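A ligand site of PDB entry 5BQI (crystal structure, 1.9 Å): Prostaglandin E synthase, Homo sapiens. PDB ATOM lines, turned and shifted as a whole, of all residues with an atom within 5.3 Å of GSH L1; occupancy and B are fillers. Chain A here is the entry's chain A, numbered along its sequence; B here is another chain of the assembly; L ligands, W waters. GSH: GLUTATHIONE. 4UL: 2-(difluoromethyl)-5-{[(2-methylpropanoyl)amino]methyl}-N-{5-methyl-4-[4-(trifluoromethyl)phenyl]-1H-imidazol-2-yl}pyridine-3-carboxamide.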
ATOM      1  N   ARG A  72      16.508   4.362  12.487  1.00  0.00           N
ATOM      2  CA  ARG A  72      15.749   4.118  11.250  1.00  0.00           C
ATOM      3  C   ARG A  72      16.040   5.193  10.209  1.00  0.00           C
ATOM      4  O   ARG A  72      16.140   4.883   9.018  1.00  0.00           O
ATOM      5  CB  ARG A  72      14.223   4.051  11.522  1.00  0.00           C
ATOM      6  CG  ARG A  72      13.773   2.796  12.258  1.00  0.00           C
ATOM      7  CD  ARG A  72      12.256   2.588  12.181  1.00  0.00           C
ATOM      8  NE  ARG A  72      11.520   3.665  12.865  1.00  0.00           N
ATOM      9  CZ  ARG A  72      11.302   3.731  14.177  1.00  0.00           C
ATOM     10  NH1 ARG A  72      11.767   2.778  14.992  1.00  0.00           N
ATOM     11  NH2 ARG A  72      10.620   4.750  14.689  1.00  0.00           N
ATOM     12  N   ALA A  73      16.167   6.445  10.635  1.00  0.00           N
ATOM     13  CA  ALA A  73      16.450   7.539   9.702  1.00  0.00           C
ATOM     14  C   ALA A  73      17.826   7.334   9.078  1.00  0.00           C
ATOM     15  O   ALA A  73      18.006   7.497   7.865  1.00  0.00           O
ATOM     16  CB  ALA A  73      16.370   8.890  10.403  1.00  0.00           C
ATOM     17  N   ARG A  75      19.461   4.453   8.865  1.00  0.00           N
ATOM     18  CA  ARG A  75      19.412   3.278   8.000  1.00  0.00           C
ATOM     19  C   ARG A  75      18.764   3.585   6.641  1.00  0.00           C
ATOM     20  O   ARG A  75      19.228   3.146   5.587  1.00  0.00           O
ATOM     21  CB  ARG A  75      18.711   2.097   8.687  1.00  0.00           C
ATOM     22  CG  ARG A  75      18.538   0.917   7.727  1.00  0.00           C
ATOM     23  CD  ARG A  75      17.898  -0.305   8.335  1.00  0.00           C
ATOM     24  NE  ARG A  75      17.594  -1.260   7.271  1.00  0.00           N
ATOM     25  CZ  ARG A  75      17.481  -2.579   7.409  1.00  0.00           C
ATOM     26  NH1 ARG A  75      17.220  -3.326   6.349  1.00  0.00           N
ATOM     27  NH2 ARG A  75      17.645  -3.153   8.591  1.00  0.00           N
ATOM     28  N   ASN A  76      17.670   4.333   6.656  1.00  0.00           N
ATOM     29  CA  ASN A  76      17.047   4.720   5.406  1.00  0.00           C
ATOM     30  C   ASN A  76      18.005   5.562   4.522  1.00  0.00           C
ATOM     31  O   ASN A  76      18.057   5.365   3.305  1.00  0.00           O
ATOM     32  CB  ASN A  76      15.705   5.430   5.643  1.00  0.00           C
ATOM     33  CG  ASN A  76      14.912   5.595   4.364  1.00  0.00           C
ATOM     34  OD1 ASN A  76      15.133   6.555   3.616  1.00  0.00           O
ATOM     35  ND2 ASN A  76      14.013   4.654   4.093  1.00  0.00           N
ATOM     36  N   GLU A  79      20.220   3.170   2.785  1.00  0.00           N
ATOM     37  CA  GLU A  79      19.481   2.486   1.726  1.00  0.00           C
ATOM     38  C   GLU A  79      19.319   3.336   0.457  1.00  0.00           C
ATOM     39  O   GLU A  79      19.075   2.798  -0.616  1.00  0.00           O
ATOM     40  CB  GLU A  79      18.093   2.020   2.229  1.00  0.00           C
ATOM     41  CG  GLU A  79      18.174   0.949   3.326  1.00  0.00           C
ATOM     42  CD  GLU A  79      16.828   0.580   3.943  1.00  0.00           C
ATOM     43  OE1 GLU A  79      15.790   1.179   3.576  1.00  0.00           O
ATOM     44  OE2 GLU A  79      16.785  -0.339   4.803  1.00  0.00           O
ATOM     45  N   HIS A 115      13.356  14.438   3.958  1.00  0.00           N
ATOM     46  CA  HIS A 115      13.069  13.130   4.541  1.00  0.00           C
ATOM     47  C   HIS A 115      13.540  13.042   5.983  1.00  0.00           C
ATOM     48  O   HIS A 115      12.806  12.584   6.848  1.00  0.00           O
ATOM     49  CB  HIS A 115      13.703  12.008   3.695  1.00  0.00           C
ATOM     50  CG  HIS A 115      13.371  10.631   4.187  1.00  0.00           C
ATOM     51  ND1 HIS A 115      14.118   9.985   5.150  1.00  0.00           N
ATOM     52  CD2 HIS A 115      12.394   9.772   3.827  1.00  0.00           C
ATOM     53  CE1 HIS A 115      13.609   8.784   5.362  1.00  0.00           C
ATOM     54  NE2 HIS A 115      12.564   8.619   4.570  1.00  0.00           N
ATOM     55  N   TYR A 119      11.314  12.717   9.237  1.00  0.00           N
ATOM     56  CA  TYR A 119      11.480  11.541  10.086  1.00  0.00           C
ATOM     57  C   TYR A 119      11.727  11.924  11.544  1.00  0.00           C
ATOM     58  O   TYR A 119      10.997  11.497  12.452  1.00  0.00           O
ATOM     59  CB  TYR A 119      12.632  10.643   9.597  1.00  0.00           C
ATOM     60  CG  TYR A 119      12.337   9.168   9.767  1.00  0.00           C
ATOM     61  CD1 TYR A 119      11.406   8.723  10.702  1.00  0.00           C
ATOM     62  CD2 TYR A 119      12.982   8.213   8.978  1.00  0.00           C
ATOM     63  CE1 TYR A 119      11.108   7.382  10.851  1.00  0.00           C
ATOM     64  CE2 TYR A 119      12.698   6.858   9.117  1.00  0.00           C
ATOM     65  CZ  TYR A 119      11.763   6.454  10.054  1.00  0.00           C
ATOM     66  OH  TYR A 119      11.444   5.126  10.205  1.00  0.00           O
ATOM     67  N   ARG A 128       6.809  12.031   5.071  1.00  0.00           N
ATOM     68  CA  ARG A 128       8.065  11.291   4.955  1.00  0.00           C
ATOM     69  C   ARG A 128       8.051  10.376   3.728  1.00  0.00           C
ATOM     70  O   ARG A 128       9.033  10.285   2.978  1.00  0.00           O
ATOM     71  CB  ARG A 128       8.353  10.468   6.213  1.00  0.00           C
ATOM     72  CG  ARG A 128       9.802   9.947   6.272  1.00  0.00           C
ATOM     73  CD  ARG A 128       9.954   8.807   7.274  1.00  0.00           C
ATOM     74  NE  ARG A 128       9.235   7.597   6.859  1.00  0.00           N
ATOM     75  CZ  ARG A 128       8.123   7.123   7.419  1.00  0.00           C
ATOM     76  NH1 ARG A 128       7.552   7.722   8.477  1.00  0.00           N
ATOM     77  NH2 ARG A 128       7.586   6.027   6.927  1.00  0.00           N
ATOM     78  N   SER A 129       6.932   9.691   3.526  1.00  0.00           N
ATOM     79  CA  SER A 129       6.825   8.718   2.455  1.00  0.00           C
ATOM     80  C   SER A 129       6.926   9.399   1.095  1.00  0.00           C
ATOM     81  O   SER A 129       7.561   8.885   0.162  1.00  0.00           O
ATOM     82  CB  SER A 129       5.545   7.902   2.605  1.00  0.00           C
ATOM     83  OG  SER A 129       5.515   6.829   1.693  1.00  0.00           O
ATOM     84  N   TYR A 132      10.583  10.475   0.391  1.00  0.00           N
ATOM     85  CA  TYR A 132      11.310   9.293  -0.040  1.00  0.00           C
ATOM     86  C   TYR A 132      11.094   9.006  -1.525  1.00  0.00           C
ATOM     87  O   TYR A 132      12.031   8.761  -2.270  1.00  0.00           O
ATOM     88  CB  TYR A 132      10.874   8.071   0.775  1.00  0.00           C
ATOM     89  CG  TYR A 132      11.360   6.765   0.213  1.00  0.00           C
ATOM     90  CD1 TYR A 132      12.658   6.310   0.468  1.00  0.00           C
ATOM     91  CD2 TYR A 132      10.537   5.986  -0.592  1.00  0.00           C
ATOM     92  CE1 TYR A 132      13.108   5.117  -0.057  1.00  0.00           C
ATOM     93  CE2 TYR A 132      10.980   4.790  -1.123  1.00  0.00           C
ATOM     94  CZ  TYR A 132      12.267   4.362  -0.852  1.00  0.00           C
ATOM     95  OH  TYR A 132      12.711   3.165  -1.369  1.00  0.00           O
ATOM     96  N   ALA B  33      13.208  -2.771  -1.446  1.00  0.00           N
ATOM     97  CA  ALA B  33      12.579  -1.660  -0.708  1.00  0.00           C
ATOM     98  C   ALA B  33      11.088  -1.548  -0.994  1.00  0.00           C
ATOM     99  O   ALA B  33      10.292  -1.341  -0.080  1.00  0.00           O
ATOM    100  CB  ALA B  33      13.269  -0.329  -1.032  1.00  0.00           C
ATOM    101  N   THR B  36       9.280  -4.439   0.582  1.00  0.00           N
ATOM    102  CA  THR B  36       9.199  -4.211   2.030  1.00  0.00           C
ATOM    103  C   THR B  36       7.994  -3.298   2.341  1.00  0.00           C
ATOM    104  O   THR B  36       7.168  -3.631   3.192  1.00  0.00           O
ATOM    105  CB  THR B  36      10.496  -3.574   2.597  1.00  0.00           C
ATOM    106  OG1 THR B  36      11.628  -4.407   2.254  1.00  0.00           O
ATOM    107  CG2 THR B  36      10.429  -3.412   4.119  1.00  0.00           C
ATOM    108  N   GLY B  37       7.889  -2.182   1.604  1.00  0.00           N
ATOM    109  CA  GLY B  37       6.760  -1.254   1.780  1.00  0.00           C
ATOM    110  C   GLY B  37       5.403  -1.905   1.546  1.00  0.00           C
ATOM    111  O   GLY B  37       4.442  -1.648   2.280  1.00  0.00           O
ATOM    112  N   ARG B  40       4.585  -4.138   4.532  1.00  0.00           N
ATOM    113  CA  ARG B  40       4.134  -3.288   5.646  1.00  0.00           C
ATOM    114  C   ARG B  40       2.666  -2.889   5.491  1.00  0.00           C
ATOM    115  O   ARG B  40       1.899  -2.970   6.432  1.00  0.00           O
ATOM    116  CB  ARG B  40       4.991  -2.019   5.765  1.00  0.00           C
ATOM    117  CG  ARG B  40       6.408  -2.253   6.274  1.00  0.00           C
ATOM    118  CD  ARG B  40       7.057  -0.917   6.652  1.00  0.00           C
ATOM    119  NE  ARG B  40       8.389  -1.075   7.237  1.00  0.00           N
ATOM    120  CZ  ARG B  40       8.622  -1.436   8.499  1.00  0.00           C
ATOM    121  NH1 ARG B  40       7.617  -1.708   9.335  1.00  0.00           N
ATOM    122  NH2 ARG B  40       9.875  -1.539   8.916  1.00  0.00           N
ATOM    123  N   ALA B  47       6.581   0.825  11.344  1.00  0.00           N
ATOM    124  CA  ALA B  47       7.643   1.082  12.308  1.00  0.00           C
ATOM    125  C   ALA B  47       7.365   2.353  13.103  1.00  0.00           C
ATOM    126  O   ALA B  47       7.893   2.534  14.204  1.00  0.00           O
ATOM    127  CB  ALA B  47       8.983   1.168  11.601  1.00  0.00           C
ATOM    128  N   ASN B  48       6.528   3.241  12.551  1.00  0.00           N
ATOM    129  CA  ASN B  48       6.289   4.548  13.152  1.00  0.00           C
ATOM    130  C   ASN B  48       4.822   4.767  13.515  1.00  0.00           C
ATOM    131  O   ASN B  48       3.945   4.416  12.727  1.00  0.00           O
ATOM    132  CB  ASN B  48       6.747   5.650  12.194  1.00  0.00           C
ATOM    133  CG  ASN B  48       8.189   5.490  11.786  1.00  0.00           C
ATOM    134  OD1 ASN B  48       9.096   5.653  12.606  1.00  0.00           O
ATOM    135  ND2 ASN B  48       8.414   5.123  10.531  1.00  0.00           N
ATOM    136  N   LEU B  71      13.624  -6.757   5.720  1.00  0.00           N
ATOM    137  CA  LEU B  71      14.655  -5.853   6.233  1.00  0.00           C
ATOM    138  C   LEU B  71      16.011  -6.541   6.308  1.00  0.00           C
ATOM    139  O   LEU B  71      17.014  -5.930   5.992  1.00  0.00           O
ATOM    140  CB  LEU B  71      14.264  -5.299   7.619  1.00  0.00           C
ATOM    141  CG  LEU B  71      13.114  -4.268   7.652  1.00  0.00           C
ATOM    142  CD1 LEU B  71      12.735  -3.958   9.098  1.00  0.00           C
ATOM    143  CD2 LEU B  71      13.511  -2.984   6.929  1.00  0.00           C
ATOM    144  N   HIS B  74      17.426  -6.817   2.774  1.00  0.00           N
ATOM    145  CA  HIS B  74      17.888  -5.506   2.338  1.00  0.00           C
ATOM    146  C   HIS B  74      19.216  -5.177   3.030  1.00  0.00           C
ATOM    147  O   HIS B  74      20.139  -4.684   2.390  1.00  0.00           O
ATOM    148  CB  HIS B  74      16.848  -4.427   2.660  1.00  0.00           C
ATOM    149  CG  HIS B  74      16.995  -3.176   1.854  1.00  0.00           C
ATOM    150  ND1 HIS B  74      15.977  -2.247   1.742  1.00  0.00           N
ATOM    151  CD2 HIS B  74      18.026  -2.691   1.132  1.00  0.00           C
ATOM    152  CE1 HIS B  74      16.387  -1.242   0.984  1.00  0.00           C
ATOM    153  NE2 HIS B  74      17.622  -1.490   0.593  1.00  0.00           N
HETATM  154  N1  GSH L   1      13.421  -0.266   4.633  1.00  0.00           N
HETATM  155  CA1 GSH L   1      12.219   0.564   4.285  1.00  0.00           C
HETATM  156  C1  GSH L   1      11.076   0.371   5.252  1.00  0.00           C
HETATM  157  O11 GSH L   1      10.169   1.218   5.267  1.00  0.00           O
HETATM  158  O12 GSH L   1      11.069  -0.603   6.035  1.00  0.00           O
HETATM  159  CB1 GSH L   1      11.793   0.263   2.849  1.00  0.00           C
HETATM  160  CG1 GSH L   1      10.773   1.225   2.233  1.00  0.00           C
HETATM  161  CD1 GSH L   1      11.137   2.686   2.439  1.00  0.00           C
HETATM  162  OE1 GSH L   1      12.292   3.075   2.311  1.00  0.00           O
HETATM  163  N2  GSH L   1      10.130   3.501   2.775  1.00  0.00           N
HETATM  164  CA2 GSH L   1      10.309   4.913   3.047  1.00  0.00           C
HETATM  165  C2  GSH L   1      10.692   5.206   4.487  1.00  0.00           C
HETATM  166  O2  GSH L   1      10.866   6.352   4.861  1.00  0.00           O
HETATM  167  CB2 GSH L   1       9.006   5.641   2.698  1.00  0.00           C
HETATM  168  SG2 GSH L   1       7.612   5.059   3.701  1.00  0.00           S
HETATM  169  N3  GSH L   1      10.828   4.153   5.302  1.00  0.00           N
HETATM  170  CA3 GSH L   1      11.068   4.314   6.721  1.00  0.00           C
HETATM  171  C3  GSH L   1      12.318   3.584   7.190  1.00  0.00           C
HETATM  172  O31 GSH L   1      13.119   3.117   6.349  1.00  0.00           O
HETATM  173  O32 GSH L   1      12.486   3.485   8.413  1.00  0.00           O
HETATM  174  O1  4UL L   2       5.412   1.430   0.170  1.00  0.00           O
HETATM  175  C7  4UL L   2       3.389  10.789  -4.407  1.00  0.00           C
HETATM  176  C6  4UL L   2       4.151   9.737  -3.904  1.00  0.00           C
HETATM  177  C1  4UL L   2       0.825   8.425  -0.362  1.00  0.00           C
HETATM  178  N1  4UL L   2       0.938   7.580   0.727  1.00  0.00           N
HETATM  179  C5  4UL L   2       3.705   8.995  -2.817  1.00  0.00           C
HETATM  180  C4  4UL L   2       2.478   9.294  -2.211  1.00  0.00           C
HETATM  181  C3  4UL L   2       2.026   8.530  -1.033  1.00  0.00           C
HETATM  182  C2  4UL L   2      -0.483   9.056  -0.665  1.00  0.00           C
HETATM  183  F4  4UL L   2       1.280   6.198   5.718  1.00  0.00           F
HETATM  184  C22 4UL L   2       2.645   6.206   5.738  1.00  0.00           C
HETATM  185  F3  4UL L   2       3.003   7.362   5.127  1.00  0.00           F
HETATM  186  C13 4UL L   2       3.226   5.035   4.924  1.00  0.00           C
HETATM  187  N3  4UL L   2       4.008   4.187   5.611  1.00  0.00           N
HETATM  188  C14 4UL L   2       4.560   3.153   4.955  1.00  0.00           C
HETATM  189  C15 4UL L   2       4.371   2.899   3.612  1.00  0.00           C
HETATM  190  C17 4UL L   2       5.044   1.737   2.924  1.00  0.00           C
HETATM  191  N4  4UL L   2       6.210   2.146   2.149  1.00  0.00           N
HETATM  192  C18 4UL L   2       6.245   2.063   0.811  1.00  0.00           C
HETATM  193  C19 4UL L   2       7.398   2.778   0.137  1.00  0.00           C
HETATM  194  C21 4UL L   2       8.309   1.787  -0.589  1.00  0.00           C
HETATM  195  C20 4UL L   2       6.876   3.861  -0.809  1.00  0.00           C
HETATM  196  C16 4UL L   2       3.582   3.790   2.898  1.00  0.00           C
HETATM  197  C12 4UL L   2       2.983   4.869   3.539  1.00  0.00           C
HETATM  198  C11 4UL L   2       2.118   5.769   2.706  1.00  0.00           C
HETATM  199  O   4UL L   2       0.933   5.942   2.968  1.00  0.00           O
HETATM  200  N2  4UL L   2       2.740   6.360   1.631  1.00  0.00           N
HETATM  201  C   4UL L   2       2.210   7.216   0.697  1.00  0.00           C
HETATM  202  N   4UL L   2       2.910   7.751  -0.331  1.00  0.00           N
HETATM  203  C9  4UL L   2       1.739  10.366  -2.701  1.00  0.00           C
HETATM  204  C8  4UL L   2       2.187  11.087  -3.796  1.00  0.00           C
HETATM  205  C10 4UL L   2       3.877  11.580  -5.573  1.00  0.00           C
HETATM  206  F2  4UL L   2       5.206  11.667  -5.625  1.00  0.00           F
HETATM  207  F1  4UL L   2       3.497  11.064  -6.738  1.00  0.00           F
HETATM  208  F   4UL L   2       3.441  12.838  -5.566  1.00  0.00           F
HETATM  209  O   HOH W   1      15.140   2.275   8.129  1.00  0.00           O
HETATM  210  O   HOH W   2      12.269   0.529   9.059  1.00  0.00           O
HETATM  211  O   HOH W   3      14.651   2.169   1.437  1.00  0.00           O
HETATM  212  O   HOH W   4       7.763   2.358   5.281  1.00  0.00           O
HETATM  213  O   HOH W   5      13.740  -2.681   3.214  1.00  0.00           O
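Residues that only touch GSH L1: Arg 72, Tyr 132, Ala 33 of chain B, Thr 36 of chain B and Leu 71 of chain B. Hydrophobic or aromatic side chains that line GSH L1: His 115, Tyr 119, Tyr 132 and Leu 71 of chain B. Within 4 Å of GSH L1: Arg 72, Asn 76, Glu 79, His 115, Tyr 119, Arg 128, Ser 129, Tyr 132, Ala 33 of chain B, Thr 36 of chain B, Arg 40 of chain B and Leu 71 of chain B. Along chain A the residues within 4 Å of GSH L1 span positions 72 to 132. The nearest printed residue that does not touch GSH L1 is His 74 of chain B (4.3 Å).
N4 of 4UL L2 sits close to SG2 of GSH L1.
The side-chain amide nitrogen of Asn 76 lies within hydrogen-bond range of an oxygen (O31) of GSH L1 (2.9 Å). NE2 of His 115 is in hydrogen-bond range of O2 of GSH L1, 2.8 Å away. The side-chain hydroxyl (OH) of Tyr 119 lies within hydrogen-bond range of an oxygen (O32) of GSH L1. An oxygen (O12) of GSH L1 lies within salt-bridge range of the guanidinium group (NE) of Arg 40 of chain B, 3.0 Å away. The guanidinium group (NE) of Arg 128 sits at hydrogen-bond distance from an oxygen (O2) of GSH L1, 2.9 Å away. The side-chain hydroxyl of Ser 129 sits close to a sulfur (SG2) of GSH L1. A nitrogen (N1) of GSH L1 lies within salt-bridge range of the side-chain carboxylate (OE1) of Glu 79 (3.0 Å). The side-chain hydroxyl of Ser 129 sits at hydrogen-bond distance from a nitrogen (N2) of 4UL L2 (2.8 Å).
Water W3 bridges OE1 of Glu 79 and OE1 of GSH L1. Water W5 lies within hydrogen-bond range of a ring nitrogen (ND1) of His 74 of chain B (2.7 Å), a nitrogen (N1) of GSH L1 (2.8 Å) and the side-chain hydroxyl (OG1) of Thr 36 of chain B (2.9 Å). Water W1 bridges an oxygen (O31) of GSH L1 (2.8 Å) and the backbone carbonyl oxygen of Arg 72 (2.9 Å). Water W2 bridges O32 of GSH L1 (3.0 Å) and NH2 of Arg 40 of chain B (3.2 Å).
OE2 of Glu 79 lies within salt-bridge range of NE of Arg 75, at 2.8 Å. The side-chain hydroxyl (OH) of Tyr 119 lies within hydrogen-bond range of the side-chain amide nitrogen (ND2) of Asn 48 of chain B (3.0 Å). NH1 of Arg 128 sits close to ND2 of Asn 48 of chain B (3.4 Å). The backbone carbonyl oxygen (O) of Leu 71 of chain B is in hydrogen-bond range of the guanidinium group (NH1) of Arg 75 (2.6 Å). The side-chain hydroxyl (OH) of Tyr 119 lies within hydrogen-bond range of the guanidinium group (NE) of Arg 72 (3.0 Å). The guanidinium group (NH2) of Arg 72 sits at hydrogen-bond distance from the side-chain amide oxygen (OD1) of Asn 48 of chain B, at 2.7 Å. OD1 of Asn 76 sits close to NE2 of His 115 (3.4 Å).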
